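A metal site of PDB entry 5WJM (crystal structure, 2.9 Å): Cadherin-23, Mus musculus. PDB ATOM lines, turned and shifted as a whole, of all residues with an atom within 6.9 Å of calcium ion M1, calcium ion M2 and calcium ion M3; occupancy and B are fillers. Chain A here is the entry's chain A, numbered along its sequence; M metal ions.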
ATOM      1  N   GLU A  19     -16.633  20.496   4.733  1.00  0.00           N
ATOM      2  CA  GLU A  19     -16.095  21.682   5.389  1.00  0.00           C
ATOM      3  C   GLU A  19     -17.148  22.277   6.336  1.00  0.00           C
ATOM      4  O   GLU A  19     -18.347  22.069   6.164  1.00  0.00           O
ATOM      5  CB  GLU A  19     -15.576  22.737   4.372  1.00  0.00           C
ATOM      6  CG  GLU A  19     -16.614  23.358   3.432  1.00  0.00           C
ATOM      7  CD  GLU A  19     -16.149  24.626   2.691  1.00  0.00           C
ATOM      8  OE1 GLU A  19     -15.217  25.344   3.099  1.00  0.00           O
ATOM      9  OE2 GLU A  19     -16.752  24.932   1.648  1.00  0.00           O
ATOM     10  N   GLY A  20     -16.672  22.987   7.358  1.00  0.00           N
ATOM     11  CA  GLY A  20     -17.565  23.698   8.307  1.00  0.00           C
ATOM     12  C   GLY A  20     -18.152  22.824   9.405  1.00  0.00           C
ATOM     13  O   GLY A  20     -18.953  23.293  10.219  1.00  0.00           O
ATOM     14  N   LEU A  72     -12.849  21.810   8.983  1.00  0.00           N
ATOM     15  CA  LEU A  72     -12.073  21.888   7.740  1.00  0.00           C
ATOM     16  C   LEU A  72     -12.605  23.027   6.819  1.00  0.00           C
ATOM     17  O   LEU A  72     -13.720  23.500   7.008  1.00  0.00           O
ATOM     18  CB  LEU A  72     -12.076  20.541   7.010  1.00  0.00           C
ATOM     19  CG  LEU A  72     -11.501  19.323   7.736  1.00  0.00           C
ATOM     20  CD1 LEU A  72     -11.597  18.085   6.870  1.00  0.00           C
ATOM     21  CD2 LEU A  72     -10.049  19.515   8.109  1.00  0.00           C
ATOM     22  N   ASP A  73     -11.780  23.438   5.845  1.00  0.00           N
ATOM     23  CA  ASP A  73     -12.097  24.507   4.870  1.00  0.00           C
ATOM     24  C   ASP A  73     -11.545  24.160   3.470  1.00  0.00           C
ATOM     25  O   ASP A  73     -10.350  24.212   3.231  1.00  0.00           O
ATOM     26  CB  ASP A  73     -11.524  25.839   5.367  1.00  0.00           C
ATOM     27  CG  ASP A  73     -11.610  26.983   4.308  1.00  0.00           C
ATOM     28  OD1 ASP A  73     -12.640  27.089   3.574  1.00  0.00           O
ATOM     29  OD2 ASP A  73     -10.649  27.796   4.220  1.00  0.00           O
ATOM     30  N   ARG A  74     -12.440  23.840   2.543  1.00  0.00           N
ATOM     31  CA  ARG A  74     -12.060  23.440   1.183  1.00  0.00           C
ATOM     32  C   ARG A  74     -11.271  24.479   0.392  1.00  0.00           C
ATOM     33  O   ARG A  74     -10.433  24.142  -0.466  1.00  0.00           O
ATOM     34  CB  ARG A  74     -13.302  23.089   0.397  1.00  0.00           C
ATOM     35  CG  ARG A  74     -13.020  22.245  -0.823  1.00  0.00           C
ATOM     36  CD  ARG A  74     -14.246  22.183  -1.694  1.00  0.00           C
ATOM     37  NE  ARG A  74     -14.518  23.531  -2.201  1.00  0.00           N
ATOM     38  CZ  ARG A  74     -13.960  24.081  -3.275  1.00  0.00           C
ATOM     39  NH1 ARG A  74     -13.123  23.395  -4.044  1.00  0.00           N
ATOM     40  NH2 ARG A  74     -14.267  25.317  -3.608  1.00  0.00           N
ATOM     41  N   GLU A  75     -11.558  25.758   0.639  1.00  0.00           N
ATOM     42  CA  GLU A  75     -10.878  26.855  -0.069  1.00  0.00           C
ATOM     43  C   GLU A  75      -9.380  27.065   0.344  1.00  0.00           C
ATOM     44  O   GLU A  75      -8.629  27.724  -0.401  1.00  0.00           O
ATOM     45  CB  GLU A  75     -11.667  28.170   0.096  1.00  0.00           C
ATOM     46  CG  GLU A  75     -12.975  28.244  -0.691  1.00  0.00           C
ATOM     47  CD  GLU A  75     -14.162  27.489  -0.069  1.00  0.00           C
ATOM     48  OE1 GLU A  75     -14.831  26.748  -0.828  1.00  0.00           O
ATOM     49  OE2 GLU A  75     -14.479  27.645   1.142  1.00  0.00           O
ATOM     50  N   THR A  76      -8.937  26.524   1.520  1.00  0.00           N
ATOM     51  CA  THR A  76      -7.510  26.525   1.881  1.00  0.00           C
ATOM     52  C   THR A  76      -6.893  25.149   1.608  1.00  0.00           C
ATOM     53  O   THR A  76      -5.811  25.061   1.032  1.00  0.00           O
ATOM     54  CB  THR A  76      -7.212  27.034   3.319  1.00  0.00           C
ATOM     55  OG1 THR A  76      -7.949  26.292   4.261  1.00  0.00           O
ATOM     56  CG2 THR A  76      -7.573  28.536   3.503  1.00  0.00           C
ATOM     57  N   LEU A 105     -15.394  17.939   1.078  1.00  0.00           N
ATOM     58  CA  LEU A 105     -16.616  18.274   0.336  1.00  0.00           C
ATOM     59  C   LEU A 105     -17.033  19.724   0.594  1.00  0.00           C
ATOM     60  O   LEU A 105     -17.031  20.192   1.745  1.00  0.00           O
ATOM     61  CB  LEU A 105     -17.791  17.372   0.720  1.00  0.00           C
ATOM     62  CG  LEU A 105     -17.785  15.870   0.398  1.00  0.00           C
ATOM     63  CD1 LEU A 105     -19.035  15.239   1.031  1.00  0.00           C
ATOM     64  CD2 LEU A 105     -17.705  15.550  -1.089  1.00  0.00           C
ATOM     65  N   ASP A 106     -17.428  20.399  -0.485  1.00  0.00           N
ATOM     66  CA  ASP A 106     -17.704  21.840  -0.493  1.00  0.00           C
ATOM     67  C   ASP A 106     -19.039  22.179   0.151  1.00  0.00           C
ATOM     68  O   ASP A 106     -19.987  21.474  -0.065  1.00  0.00           O
ATOM     69  CB  ASP A 106     -17.758  22.298  -1.947  1.00  0.00           C
ATOM     70  CG  ASP A 106     -17.942  23.773  -2.086  1.00  0.00           C
ATOM     71  OD1 ASP A 106     -17.195  24.529  -1.436  1.00  0.00           O
ATOM     72  OD2 ASP A 106     -18.805  24.192  -2.882  1.00  0.00           O
ATOM     73  N   ILE A 107     -19.113  23.266   0.918  1.00  0.00           N
ATOM     74  CA  ILE A 107     -20.415  23.888   1.221  1.00  0.00           C
ATOM     75  C   ILE A 107     -20.437  25.257   0.547  1.00  0.00           C
ATOM     76  O   ILE A 107     -19.394  25.706   0.044  1.00  0.00           O
ATOM     77  CB  ILE A 107     -20.741  23.985   2.740  1.00  0.00           C
ATOM     78  CG1 ILE A 107     -19.978  25.131   3.431  1.00  0.00           C
ATOM     79  CG2 ILE A 107     -20.525  22.635   3.420  1.00  0.00           C
ATOM     80  CD1 ILE A 107     -20.124  25.179   4.940  1.00  0.00           C
ATOM     81  N   ASN A 108     -21.609  25.898   0.531  1.00  0.00           N
ATOM     82  CA  ASN A 108     -21.755  27.210  -0.095  1.00  0.00           C
ATOM     83  C   ASN A 108     -21.501  28.315   0.929  1.00  0.00           C
ATOM     84  O   ASN A 108     -22.412  28.848   1.562  1.00  0.00           O
ATOM     85  CB  ASN A 108     -23.130  27.348  -0.739  1.00  0.00           C
ATOM     86  CG  ASN A 108     -23.220  28.548  -1.668  1.00  0.00           C
ATOM     87  OD1 ASN A 108     -22.294  28.833  -2.435  1.00  0.00           O
ATOM     88  ND2 ASN A 108     -24.338  29.254  -1.603  1.00  0.00           N
ATOM     89  N   ASP A 109     -20.240  28.648   1.089  1.00  0.00           N
ATOM     90  CA  ASP A 109     -19.808  29.555   2.111  1.00  0.00           C
ATOM     91  C   ASP A 109     -19.094  30.771   1.510  1.00  0.00           C
ATOM     92  O   ASP A 109     -18.358  31.479   2.213  1.00  0.00           O
ATOM     93  CB  ASP A 109     -18.962  28.796   3.179  1.00  0.00           C
ATOM     94  CG  ASP A 109     -17.678  28.132   2.628  1.00  0.00           C
ATOM     95  OD1 ASP A 109     -17.718  27.477   1.567  1.00  0.00           O
ATOM     96  OD2 ASP A 109     -16.604  28.260   3.254  1.00  0.00           O
ATOM     97  N   ASN A 110     -19.331  31.017   0.219  1.00  0.00           N
ATOM     98  CA  ASN A 110     -18.728  32.142  -0.502  1.00  0.00           C
ATOM     99  C   ASN A 110     -19.776  32.784  -1.432  1.00  0.00           C
ATOM    100  O   ASN A 110     -20.354  32.106  -2.294  1.00  0.00           O
ATOM    101  CB  ASN A 110     -17.524  31.718  -1.342  1.00  0.00           C
ATOM    102  CG  ASN A 110     -16.349  31.210  -0.508  1.00  0.00           C
ATOM    103  OD1 ASN A 110     -15.382  31.937  -0.268  1.00  0.00           O
ATOM    104  ND2 ASN A 110     -16.399  29.946  -0.109  1.00  0.00           N
ATOM    105  N   ASP A 111     -19.991  34.082  -1.250  1.00  0.00           N
ATOM    106  CA  ASP A 111     -20.864  34.874  -2.115  1.00  0.00           C
ATOM    107  C   ASP A 111     -20.298  34.916  -3.534  1.00  0.00           C
ATOM    108  O   ASP A 111     -19.075  34.916  -3.714  1.00  0.00           O
ATOM    109  CB  ASP A 111     -21.018  36.324  -1.572  1.00  0.00           C
ATOM    110  CG  ASP A 111     -21.915  36.422  -0.309  1.00  0.00           C
ATOM    111  OD1 ASP A 111     -22.570  35.435   0.083  1.00  0.00           O
ATOM    112  OD2 ASP A 111     -21.975  37.530   0.304  1.00  0.00           O
ATOM    113  N   PRO A 112     -21.158  34.954  -4.564  1.00  0.00           N
ATOM    114  CA  PRO A 112     -20.621  35.328  -5.874  1.00  0.00           C
ATOM    115  C   PRO A 112     -20.221  36.789  -5.853  1.00  0.00           C
ATOM    116  O   PRO A 112     -20.692  37.524  -4.997  1.00  0.00           O
ATOM    117  CB  PRO A 112     -21.798  35.068  -6.841  1.00  0.00           C
ATOM    118  CG  PRO A 112     -23.009  35.047  -5.995  1.00  0.00           C
ATOM    119  CD  PRO A 112     -22.595  34.634  -4.618  1.00  0.00           C
ATOM    120  N   ASP A 140     -16.878  32.965  -8.239  1.00  0.00           N
ATOM    121  CA  ASP A 140     -17.338  32.304  -6.990  1.00  0.00           C
ATOM    122  C   ASP A 140     -16.261  31.286  -6.532  1.00  0.00           C
ATOM    123  O   ASP A 140     -15.837  30.406  -7.289  1.00  0.00           O
ATOM    124  CB  ASP A 140     -18.699  31.634  -7.207  1.00  0.00           C
ATOM    125  CG  ASP A 140     -19.446  31.298  -5.894  1.00  0.00           C
ATOM    126  OD1 ASP A 140     -18.943  30.496  -5.070  1.00  0.00           O
ATOM    127  OD2 ASP A 140     -20.570  31.804  -5.692  1.00  0.00           O
ATOM    128  N   ALA A 141     -15.833  31.424  -5.297  1.00  0.00           N
ATOM    129  CA  ALA A 141     -14.716  30.642  -4.771  1.00  0.00           C
ATOM    130  C   ALA A 141     -15.060  29.166  -4.491  1.00  0.00           C
ATOM    131  O   ALA A 141     -14.154  28.334  -4.357  1.00  0.00           O
ATOM    132  CB  ALA A 141     -14.156  31.314  -3.517  1.00  0.00           C
ATOM    133  N   ASP A 142     -16.366  28.850  -4.405  1.00  0.00           N
ATOM    134  CA  ASP A 142     -16.848  27.482  -4.160  1.00  0.00           C
ATOM    135  C   ASP A 142     -16.613  26.614  -5.417  1.00  0.00           C
ATOM    136  O   ASP A 142     -16.015  27.082  -6.401  1.00  0.00           O
ATOM    137  CB  ASP A 142     -18.331  27.492  -3.727  1.00  0.00           C
ATOM    138  CG  ASP A 142     -18.574  28.270  -2.390  1.00  0.00           C
ATOM    139  OD1 ASP A 142     -17.834  28.064  -1.397  1.00  0.00           O
ATOM    140  OD2 ASP A 142     -19.518  29.108  -2.331  1.00  0.00           O
ATOM    141  N   SER A 143     -17.029  25.360  -5.355  1.00  0.00           N
ATOM    142  CA  SER A 143     -16.949  24.439  -6.487  1.00  0.00           C
ATOM    143  C   SER A 143     -18.324  23.896  -6.810  1.00  0.00           C
ATOM    144  O   SER A 143     -19.286  24.141  -6.060  1.00  0.00           O
ATOM    145  CB  SER A 143     -16.006  23.278  -6.165  1.00  0.00           C
ATOM    146  OG  SER A 143     -16.694  22.280  -5.413  1.00  0.00           O
ATOM    147  N   CYS A 145     -22.025  22.963  -8.093  1.00  0.00           N
ATOM    148  CA  CYS A 145     -23.258  23.758  -8.165  1.00  0.00           C
ATOM    149  C   CYS A 145     -23.205  25.020  -7.270  1.00  0.00           C
ATOM    150  O   CYS A 145     -23.933  26.003  -7.495  1.00  0.00           O
ATOM    151  CB  CYS A 145     -24.475  22.888  -7.817  1.00  0.00           C
ATOM    152  SG  CYS A 145     -24.646  22.412  -6.088  1.00  0.00           S
ATOM    153  N   ASN A 146     -22.318  25.023  -6.263  1.00  0.00           N
ATOM    154  CA  ASN A 146     -22.140  26.191  -5.369  1.00  0.00           C
ATOM    155  C   ASN A 146     -21.394  27.370  -6.003  1.00  0.00           C
ATOM    156  O   ASN A 146     -21.305  28.442  -5.389  1.00  0.00           O
ATOM    157  CB  ASN A 146     -21.400  25.777  -4.078  1.00  0.00           C
ATOM    158  CG  ASN A 146     -22.160  24.741  -3.274  1.00  0.00           C
ATOM    159  OD1 ASN A 146     -23.381  24.721  -3.260  1.00  0.00           O
ATOM    160  ND2 ASN A 146     -21.440  23.880  -2.581  1.00  0.00           N
ATOM    161  N   ALA A 147     -20.813  27.156  -7.177  1.00  0.00           N
ATOM    162  CA  ALA A 147     -20.205  28.231  -7.961  1.00  0.00           C
ATOM    163  C   ALA A 147     -20.790  28.341  -9.377  1.00  0.00           C
ATOM    164  O   ALA A 147     -20.264  29.086 -10.199  1.00  0.00           O
ATOM    165  CB  ALA A 147     -18.690  28.057  -8.015  1.00  0.00           C
ATOM    166  N   LEU A 148     -21.903  27.648  -9.640  1.00  0.00           N
ATOM    167  CA  LEU A 148     -22.597  27.761 -10.926  1.00  0.00           C
ATOM    168  C   LEU A 148     -23.480  29.000 -10.853  1.00  0.00           C
ATOM    169  O   LEU A 148     -24.444  29.027 -10.073  1.00  0.00           O
ATOM    170  CB  LEU A 148     -23.461  26.512 -11.195  1.00  0.00           C
ATOM    171  CG  LEU A 148     -24.409  26.614 -12.416  1.00  0.00           C
ATOM    172  CD1 LEU A 148     -23.615  26.858 -13.691  1.00  0.00           C
ATOM    173  CD2 LEU A 148     -25.310  25.388 -12.561  1.00  0.00           C
ATOM    174  N   LEU A 149     -23.166  30.023 -11.668  1.00  0.00           N
ATOM    175  CA  LEU A 149     -23.805  31.342 -11.551  1.00  0.00           C
ATOM    176  C   LEU A 149     -24.923  31.599 -12.566  1.00  0.00           C
ATOM    177  O   LEU A 149     -24.813  31.218 -13.738  1.00  0.00           O
ATOM    178  CB  LEU A 149     -22.746  32.440 -11.667  1.00  0.00           C
ATOM    179  CG  LEU A 149     -21.577  32.345 -10.702  1.00  0.00           C
ATOM    180  CD1 LEU A 149     -20.711  33.586 -10.795  1.00  0.00           C
ATOM    181  CD2 LEU A 149     -22.065  32.134  -9.288  1.00  0.00           C
ATOM    182  N   ASP A 193     -25.583  32.141  -7.068  1.00  0.00           N
ATOM    183  CA  ASP A 193     -25.190  30.739  -7.215  1.00  0.00           C
ATOM    184  C   ASP A 193     -26.431  29.831  -7.071  1.00  0.00           C
ATOM    185  O   ASP A 193     -27.528  30.283  -6.736  1.00  0.00           O
ATOM    186  CB  ASP A 193     -23.999  30.307  -6.309  1.00  0.00           C
ATOM    187  CG  ASP A 193     -24.161  30.714  -4.838  1.00  0.00           C
ATOM    188  OD1 ASP A 193     -25.296  30.756  -4.333  1.00  0.00           O
ATOM    189  OD2 ASP A 193     -23.140  30.990  -4.180  1.00  0.00           O
ATOM    190  N   ASN A 194     -26.227  28.555  -7.375  1.00  0.00           N
ATOM    191  CA  ASN A 194     -27.325  27.590  -7.477  1.00  0.00           C
ATOM    192  C   ASN A 194     -26.972  26.329  -6.710  1.00  0.00           C
ATOM    193  O   ASN A 194     -26.766  25.284  -7.313  1.00  0.00           O
ATOM    194  CB  ASN A 194     -27.601  27.264  -8.957  1.00  0.00           C
ATOM    195  CG  ASN A 194     -28.047  28.475  -9.737  1.00  0.00           C
ATOM    196  OD1 ASN A 194     -29.231  28.708  -9.902  1.00  0.00           O
ATOM    197  ND2 ASN A 194     -27.092  29.269 -10.205  1.00  0.00           N
ATOM    198  N   PRO A 195     -26.919  26.407  -5.367  1.00  0.00           N
ATOM    199  CA  PRO A 195     -26.657  25.216  -4.569  1.00  0.00           C
ATOM    200  C   PRO A 195     -27.820  24.241  -4.648  1.00  0.00           C
ATOM    201  O   PRO A 195     -28.890  24.629  -5.088  1.00  0.00           O
ATOM    202  CB  PRO A 195     -26.486  25.763  -3.144  1.00  0.00           C
ATOM    203  CG  PRO A 195     -27.150  27.088  -3.139  1.00  0.00           C
ATOM    204  CD  PRO A 195     -27.154  27.613  -4.548  1.00  0.00           C
ATOM    205  N   ARG A 202     -26.560  32.309  -2.384  1.00  0.00           N
ATOM    206  CA  ARG A 202     -25.975  33.629  -2.115  1.00  0.00           C
ATOM    207  C   ARG A 202     -25.931  34.452  -3.411  1.00  0.00           C
ATOM    208  O   ARG A 202     -25.878  33.880  -4.504  1.00  0.00           O
ATOM    209  CB  ARG A 202     -24.587  33.456  -1.507  1.00  0.00           C
ATOM    210  CG  ARG A 202     -24.521  32.404  -0.401  1.00  0.00           C
ATOM    211  CD  ARG A 202     -23.114  31.899  -0.115  1.00  0.00           C
ATOM    212  NE  ARG A 202     -22.510  32.674   0.972  1.00  0.00           N
ATOM    213  CZ  ARG A 202     -22.602  32.384   2.271  1.00  0.00           C
ATOM    214  NH1 ARG A 202     -23.250  31.295   2.693  1.00  0.00           N
ATOM    215  NH2 ARG A 202     -22.028  33.186   3.161  1.00  0.00           N
HETATM  216 CA    CA M   1     -20.899  30.182  -3.731  1.00  0.00          CA
HETATM  217 CA    CA M   2     -17.002  26.268  -0.188  1.00  0.00          CA
HETATM  218 CA    CA M   3     -14.685  27.552   3.467  1.00  0.00          CA
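The backbone NH (N) of Arg 202 sits at hydrogen-bond distance from the side-chain carboxylate (OD1) of Asp 193, 2.8 Å away. The side-chain carboxylate (OD1) of Asp 109 lies close to the side-chain amide nitrogen (ND2) of Asn 110. The side-chain carboxylate (OD2) of Asp 106 lies within hydrogen-bond range of the side-chain amide nitrogen (ND2) of Asn 146 (2.7 Å). The backbone NH of Arg 74 sits close to the side-chain carboxylate of Glu 19, 3.2 Å away. The side-chain hydroxyl (OG1) of Thr 76 is in hydrogen-bond range of the side-chain carboxylate (OD2) of Asp 73 (3.1 Å). OE1 of Glu 75 lies close to NH2 of Arg 74, at 3.2 Å. The backbone NH (N) of Ser 143 is in hydrogen-bond range of the side-chain carboxylate (OD2) of Asp 106, 3.3 Å away. The side-chain carboxylate (OE2) of Glu 75 lies close to the side-chain amide nitrogen (ND2) of Asn 110 (3.2 Å).
Of the 28 residues printed, 6 come within 4 Å of calcium ion M1. Along chain A the residues within 4 Å of calcium ion M1 span positions 108 to 193.
Along chain A the residues within 4 Å of calcium ion M2 span positions 19 to 142. The nearest printed residue that does not touch calcium ion M2 is Arg 74 (4.2 Å).
Of the 28 residues printed, 4 come within 4 Å of calcium ion M3. The nearest printed residue that does not touch calcium ion M3 is Arg 74 (4.4 Å).
Calcium ion M1 is bound by OD2 of Asp 142, 2.2 Å away. The side-chain amide oxygen (OD1) of Asn 108 binds calcium ion M1. OD1 of Asp 140 is bound to calcium ion M1 (2.4 Å). The side-chain carboxylate (OD2) of Asp 193 binds calcium ion M1 (2.4 Å). O of Asn 146 binds calcium ion M1 (2.4 Å). The backbone carbonyl oxygen (O) of Asn 110 binds calcium ion M1 (2.5 Å). The side-chain carboxylate (OD2) of Asp 140 is bound to calcium ion M1.
Calcium ion M2 is bound by OD1 of Asp 106 (2.1 Å), OD1 of Asp 109 (2.2 Å), OE2 of Glu 19 (2.3 Å), OE1 of Glu 75 (2.3 Å), OD1 of Asp 142 (2.3 Å) and O of Ile 107 (2.5 Å). Calcium ion M2 has six donor atoms within binding distance.
OD2 of Asp 109 binds calcium ion M3. OD1 of Asp 73 binds calcium ion M3 (2.1 Å). OE1 of Glu 19 is bound to calcium ion M3, 2.3 Å away. OE2 of Glu 75 binds calcium ion M3 (2.3 Å). Calcium ion M3 has four donor atoms within binding distance.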
